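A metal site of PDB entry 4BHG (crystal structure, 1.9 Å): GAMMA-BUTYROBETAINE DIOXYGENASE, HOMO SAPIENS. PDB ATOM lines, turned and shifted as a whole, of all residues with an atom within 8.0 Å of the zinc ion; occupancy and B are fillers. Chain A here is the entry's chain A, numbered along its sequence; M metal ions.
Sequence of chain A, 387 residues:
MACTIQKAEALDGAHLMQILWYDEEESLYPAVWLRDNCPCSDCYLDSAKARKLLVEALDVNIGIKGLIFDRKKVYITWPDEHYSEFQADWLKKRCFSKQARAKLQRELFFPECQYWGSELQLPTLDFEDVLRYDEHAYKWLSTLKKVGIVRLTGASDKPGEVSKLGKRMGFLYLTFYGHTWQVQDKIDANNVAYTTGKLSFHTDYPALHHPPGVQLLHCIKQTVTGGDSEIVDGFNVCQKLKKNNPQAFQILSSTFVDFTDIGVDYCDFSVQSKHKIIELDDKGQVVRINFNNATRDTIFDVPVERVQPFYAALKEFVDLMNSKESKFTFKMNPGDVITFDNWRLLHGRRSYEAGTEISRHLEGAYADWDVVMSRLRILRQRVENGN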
ATOM      1  N   LEU A  34      -2.392   1.078 -17.365  1.00  0.00           N
ATOM      2  CA  LEU A  34      -2.033   1.686 -16.073  1.00  0.00           C
ATOM      3  C   LEU A  34      -0.543   1.954 -15.963  1.00  0.00           C
ATOM      4  O   LEU A  34      -0.127   3.058 -15.642  1.00  0.00           O
ATOM      5  CB  LEU A  34      -2.492   0.774 -14.919  1.00  0.00           C
ATOM      6  CG  LEU A  34      -3.999   0.649 -14.729  1.00  0.00           C
ATOM      7  CD1 LEU A  34      -4.317  -0.477 -13.744  1.00  0.00           C
ATOM      8  CD2 LEU A  34      -4.619   1.945 -14.223  1.00  0.00           C
ATOM      9  N   ARG A  35       0.276   0.955 -16.273  1.00  0.00           N
ATOM     10  CA  ARG A  35       1.709   1.133 -16.203  1.00  0.00           C
ATOM     11  C   ARG A  35       2.192   2.245 -17.140  1.00  0.00           C
ATOM     12  O   ARG A  35       3.001   3.083 -16.749  1.00  0.00           O
ATOM     13  CB  ARG A  35       2.439  -0.172 -16.525  1.00  0.00           C
ATOM     14  CG  ARG A  35       3.981  -0.057 -16.485  1.00  0.00           C
ATOM     15  CD  ARG A  35       4.470   0.231 -15.080  1.00  0.00           C
ATOM     16  NE  ARG A  35       5.874   0.590 -14.963  1.00  0.00           N
ATOM     17  CZ  ARG A  35       6.366   1.812 -15.136  1.00  0.00           C
ATOM     18  NH1 ARG A  35       5.556   2.828 -15.410  1.00  0.00           N
ATOM     19  NH2 ARG A  35       7.674   2.032 -14.953  1.00  0.00           N
ATOM     20  N   ASP A  36       1.672   2.242 -18.371  1.00  0.00           N
ATOM     21  CA  ASP A  36       2.016   3.249 -19.401  1.00  0.00           C
ATOM     22  C   ASP A  36       1.707   4.662 -18.910  1.00  0.00           C
ATOM     23  O   ASP A  36       2.346   5.605 -19.333  1.00  0.00           O
ATOM     24  CB  ASP A  36       1.154   2.996 -20.652  1.00  0.00           C
ATOM     25  CG  ASP A  36       1.455   3.962 -21.772  1.00  0.00           C
ATOM     26  OD1 ASP A  36       2.632   4.157 -22.097  1.00  0.00           O
ATOM     27  OD2 ASP A  36       0.472   4.494 -22.347  1.00  0.00           O
ATOM     28  N   ASN A  37       0.693   4.759 -18.039  1.00  0.00           N
ATOM     29  CA  ASN A  37       0.182   6.058 -17.602  1.00  0.00           C
ATOM     30  C   ASN A  37       0.442   6.362 -16.136  1.00  0.00           C
ATOM     31  O   ASN A  37      -0.198   7.191 -15.533  1.00  0.00           O
ATOM     32  CB  ASN A  37      -1.281   6.181 -17.995  1.00  0.00           C
ATOM     33  CG  ASN A  37      -1.420   6.320 -19.505  1.00  0.00           C
ATOM     34  OD1 ASN A  37      -0.911   7.270 -20.089  1.00  0.00           O
ATOM     35  ND2 ASN A  37      -2.018   5.330 -20.144  1.00  0.00           N
ATOM     36  N   CYS A  38       1.488   5.729 -15.602  1.00  0.00           N
ATOM     37  CA  CYS A  38       1.963   6.068 -14.264  1.00  0.00           C
ATOM     38  C   CYS A  38       2.266   7.554 -14.160  1.00  0.00           C
ATOM     39  O   CYS A  38       3.000   8.081 -14.979  1.00  0.00           O
ATOM     40  CB  CYS A  38       3.207   5.275 -13.930  1.00  0.00           C
ATOM     41  SG  CYS A  38       3.823   5.655 -12.292  1.00  0.00           S
ATOM     42  N   PRO A  39       1.661   8.256 -13.185  1.00  0.00           N
ATOM     43  CA  PRO A  39       1.890   9.697 -13.095  1.00  0.00           C
ATOM     44  C   PRO A  39       3.084  10.089 -12.249  1.00  0.00           C
ATOM     45  O   PRO A  39       3.259  11.265 -11.976  1.00  0.00           O
ATOM     46  CB  PRO A  39       0.594  10.212 -12.483  1.00  0.00           C
ATOM     47  CG  PRO A  39       0.127   9.096 -11.628  1.00  0.00           C
ATOM     48  CD  PRO A  39       0.612   7.811 -12.265  1.00  0.00           C
ATOM     49  N   CYS A  40       3.893   9.127 -11.794  1.00  0.00           N
ATOM     50  CA  CYS A  40       5.021   9.519 -10.973  1.00  0.00           C
ATOM     51  C   CYS A  40       6.038  10.385 -11.767  1.00  0.00           C
ATOM     52  O   CYS A  40       6.030  10.434 -13.021  1.00  0.00           O
ATOM     53  CB  CYS A  40       5.725   8.274 -10.356  1.00  0.00           C
ATOM     54  SG  CYS A  40       7.013   7.537 -11.376  1.00  0.00           S
ATOM     55  N   SER A  41       6.941  11.033 -11.043  1.00  0.00           N
ATOM     56  CA  SER A  41       7.896  11.925 -11.694  1.00  0.00           C
ATOM     57  C   SER A  41       8.938  11.225 -12.596  1.00  0.00           C
ATOM     58  O   SER A  41       9.511  11.873 -13.490  1.00  0.00           O
ATOM     59  CB  SER A  41       8.563  12.843 -10.662  1.00  0.00           C
ATOM     60  OG  SER A  41       9.387  12.098  -9.811  1.00  0.00           O
ATOM     61  N   ASP A  42       9.182   9.935 -12.398  1.00  0.00           N
ATOM     62  CA  ASP A  42      10.014   9.212 -13.357  1.00  0.00           C
ATOM     63  C   ASP A  42       9.318   9.000 -14.721  1.00  0.00           C
ATOM     64  O   ASP A  42       9.978   8.996 -15.789  1.00  0.00           O
ATOM     65  CB  ASP A  42      10.416   7.842 -12.800  1.00  0.00           C
ATOM     66  CG  ASP A  42      11.372   7.948 -11.616  1.00  0.00           C
ATOM     67  OD1 ASP A  42      11.882   9.030 -11.346  1.00  0.00           O
ATOM     68  OD2 ASP A  42      11.661   6.907 -10.999  1.00  0.00           O
ATOM     69  N   CYS A  43       8.011   8.793 -14.666  1.00  0.00           N
ATOM     70  CA  CYS A  43       7.238   8.390 -15.826  1.00  0.00           C
ATOM     71  C   CYS A  43       6.589   9.547 -16.518  1.00  0.00           C
ATOM     72  O   CYS A  43       6.222   9.436 -17.690  1.00  0.00           O
ATOM     73  CB  CYS A  43       6.164   7.386 -15.396  1.00  0.00           C
ATOM     74  SG  CYS A  43       6.851   5.855 -14.778  1.00  0.00           S
ATOM     75  N   TYR A  44       6.417  10.654 -15.815  1.00  0.00           N
ATOM     76  CA  TYR A  44       5.540  11.710 -16.287  1.00  0.00           C
ATOM     77  C   TYR A  44       6.115  13.049 -15.901  1.00  0.00           C
ATOM     78  O   TYR A  44       6.404  13.287 -14.722  1.00  0.00           O
ATOM     79  CB  TYR A  44       4.171  11.546 -15.656  1.00  0.00           C
ATOM     80  CG  TYR A  44       3.084  12.391 -16.253  1.00  0.00           C
ATOM     81  CD1 TYR A  44       2.439  11.989 -17.415  1.00  0.00           C
ATOM     82  CD2 TYR A  44       2.704  13.598 -15.675  1.00  0.00           C
ATOM     83  CE1 TYR A  44       1.441  12.735 -17.972  1.00  0.00           C
ATOM     84  CE2 TYR A  44       1.685  14.365 -16.242  1.00  0.00           C
ATOM     85  CZ  TYR A  44       1.061  13.933 -17.383  1.00  0.00           C
ATOM     86  OH  TYR A  44       0.047  14.672 -17.963  1.00  0.00           O
ATOM     87  N   LEU A  53       7.964   8.168 -19.882  1.00  0.00           N
ATOM     88  CA  LEU A  53       8.127   6.731 -20.064  1.00  0.00           C
ATOM     89  C   LEU A  53       8.211   6.378 -21.545  1.00  0.00           C
ATOM     90  O   LEU A  53       7.365   6.791 -22.332  1.00  0.00           O
ATOM     91  CB  LEU A  53       6.974   5.977 -19.404  1.00  0.00           C
ATOM     92  CG  LEU A  53       7.091   4.464 -19.342  1.00  0.00           C
ATOM     93  CD1 LEU A  53       8.051   4.083 -18.208  1.00  0.00           C
ATOM     94  CD2 LEU A  53       5.710   3.833 -19.159  1.00  0.00           C
ATOM     95  N   TRP A  78       4.334  -3.003  -9.125  1.00  0.00           N
ATOM     96  CA  TRP A  78       4.596  -3.738 -10.346  1.00  0.00           C
ATOM     97  C   TRP A  78       5.675  -4.814 -10.147  1.00  0.00           C
ATOM     98  O   TRP A  78       6.452  -4.740  -9.201  1.00  0.00           O
ATOM     99  CB  TRP A  78       5.041  -2.757 -11.440  1.00  0.00           C
ATOM    100  CG  TRP A  78       3.990  -1.726 -11.735  1.00  0.00           C
ATOM    101  CD1 TRP A  78       4.013  -0.407 -11.416  1.00  0.00           C
ATOM    102  CD2 TRP A  78       2.746  -1.954 -12.390  1.00  0.00           C
ATOM    103  NE1 TRP A  78       2.865   0.202 -11.852  1.00  0.00           N
ATOM    104  CE2 TRP A  78       2.074  -0.728 -12.460  1.00  0.00           C
ATOM    105  CE3 TRP A  78       2.133  -3.092 -12.909  1.00  0.00           C
ATOM    106  CZ2 TRP A  78       0.819  -0.593 -13.050  1.00  0.00           C
ATOM    107  CZ3 TRP A  78       0.891  -2.949 -13.528  1.00  0.00           C
ATOM    108  CH2 TRP A  78       0.248  -1.709 -13.588  1.00  0.00           C
ATOM    109  N   HIS A  82       8.554  -1.159  -9.485  1.00  0.00           N
ATOM    110  CA  HIS A  82       7.986   0.182  -9.709  1.00  0.00           C
ATOM    111  C   HIS A  82       6.669   0.315  -8.947  1.00  0.00           C
ATOM    112  O   HIS A  82       5.945  -0.677  -8.716  1.00  0.00           O
ATOM    113  CB  HIS A  82       7.792   0.459 -11.213  1.00  0.00           C
ATOM    114  CG  HIS A  82       7.663   1.924 -11.547  1.00  0.00           C
ATOM    115  ND1 HIS A  82       8.748   2.750 -11.635  1.00  0.00           N
ATOM    116  CD2 HIS A  82       6.579   2.698 -11.793  1.00  0.00           C
ATOM    117  CE1 HIS A  82       8.354   3.976 -11.912  1.00  0.00           C
ATOM    118  NE2 HIS A  82       7.042   3.972 -12.032  1.00  0.00           N
ATOM    119  N   TYR A  83       6.313   1.553  -8.601  1.00  0.00           N
ATOM    120  CA  TYR A  83       5.195   1.820  -7.727  1.00  0.00           C
ATOM    121  C   TYR A  83       4.404   2.971  -8.289  1.00  0.00           C
ATOM    122  O   TYR A  83       4.991   3.966  -8.674  1.00  0.00           O
ATOM    123  CB  TYR A  83       5.711   2.193  -6.321  1.00  0.00           C
ATOM    124  CG  TYR A  83       4.670   2.799  -5.427  1.00  0.00           C
ATOM    125  CD1 TYR A  83       3.618   2.009  -4.953  1.00  0.00           C
ATOM    126  CD2 TYR A  83       4.683   4.158  -5.077  1.00  0.00           C
ATOM    127  CE1 TYR A  83       2.645   2.527  -4.135  1.00  0.00           C
ATOM    128  CE2 TYR A  83       3.698   4.701  -4.257  1.00  0.00           C
ATOM    129  CZ  TYR A  83       2.671   3.861  -3.786  1.00  0.00           C
ATOM    130  OH  TYR A  83       1.638   4.292  -2.960  1.00  0.00           O
ATOM    131  N   SER A  84       3.079   2.824  -8.365  1.00  0.00           N
ATOM    132  CA  SER A  84       2.201   3.845  -8.942  1.00  0.00           C
ATOM    133  C   SER A  84       0.994   4.171  -8.084  1.00  0.00           C
ATOM    134  O   SER A  84       0.433   3.273  -7.462  1.00  0.00           O
ATOM    135  CB  SER A  84       1.661   3.379 -10.319  1.00  0.00           C
ATOM    136  OG  SER A  84       2.686   3.020 -11.225  1.00  0.00           O
ATOM    137  N   GLU A  85       0.553   5.432  -8.115  1.00  0.00           N
ATOM    138  CA  GLU A  85      -0.707   5.847  -7.507  1.00  0.00           C
ATOM    139  C   GLU A  85      -1.619   6.476  -8.529  1.00  0.00           C
ATOM    140  O   GLU A  85      -1.199   7.344  -9.329  1.00  0.00           O
ATOM    141  CB  GLU A  85      -0.449   6.840  -6.369  1.00  0.00           C
ATOM    142  CG  GLU A  85       0.564   6.364  -5.350  1.00  0.00           C
ATOM    143  CD  GLU A  85       0.666   7.258  -4.124  1.00  0.00           C
ATOM    144  OE1 GLU A  85       0.161   8.392  -4.159  1.00  0.00           O
ATOM    145  OE2 GLU A  85       1.281   6.814  -3.127  1.00  0.00           O
ATOM    146  N   PHE A  86      -2.883   6.062  -8.505  1.00  0.00           N
ATOM    147  CA  PHE A  86      -3.903   6.638  -9.388  1.00  0.00           C
ATOM    148  C   PHE A  86      -5.088   7.185  -8.597  1.00  0.00           C
ATOM    149  O   PHE A  86      -5.588   6.524  -7.662  1.00  0.00           O
ATOM    150  CB  PHE A  86      -4.411   5.584 -10.374  1.00  0.00           C
ATOM    151  CG  PHE A  86      -3.319   4.945 -11.197  1.00  0.00           C
ATOM    152  CD1 PHE A  86      -2.908   5.542 -12.389  1.00  0.00           C
ATOM    153  CD2 PHE A  86      -2.701   3.778 -10.793  1.00  0.00           C
ATOM    154  CE1 PHE A  86      -1.915   4.969 -13.152  1.00  0.00           C
ATOM    155  CE2 PHE A  86      -1.700   3.201 -11.551  1.00  0.00           C
ATOM    156  CZ  PHE A  86      -1.312   3.787 -12.742  1.00  0.00           C
HETATM  157 ZN    ZN M   1       6.095   5.749 -12.596  1.00  0.00          ZN
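Four residues have an atom within 4 Å of the zinc ion: Cys 38, Cys 40, Cys 43 and His 82.
O of Cys 43 lies within hydrogen-bond range of N of Leu 53 (3.1 Å). The side-chain sulfur (SG) of Cys 38 lies close to the side-chain hydroxyl (OG) of Ser 84. The side-chain sulfur (SG) of Cys 40 sits close to the backbone NH (N) of Asp 42, 3.4 Å away. The side-chain sulfur (SG) of Cys 43 lies close to the guanidinium group (NH1) of Arg 35, 3.4 Å away.
The zinc ion is bound by a ring nitrogen (NE2) of His 82, the side-chain sulfur (SG) of Cys 38, the side-chain sulfur (SG) of Cys 43 and the side-chain sulfur (SG) of Cys 40. The zinc ion has four donor atoms within binding distance.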
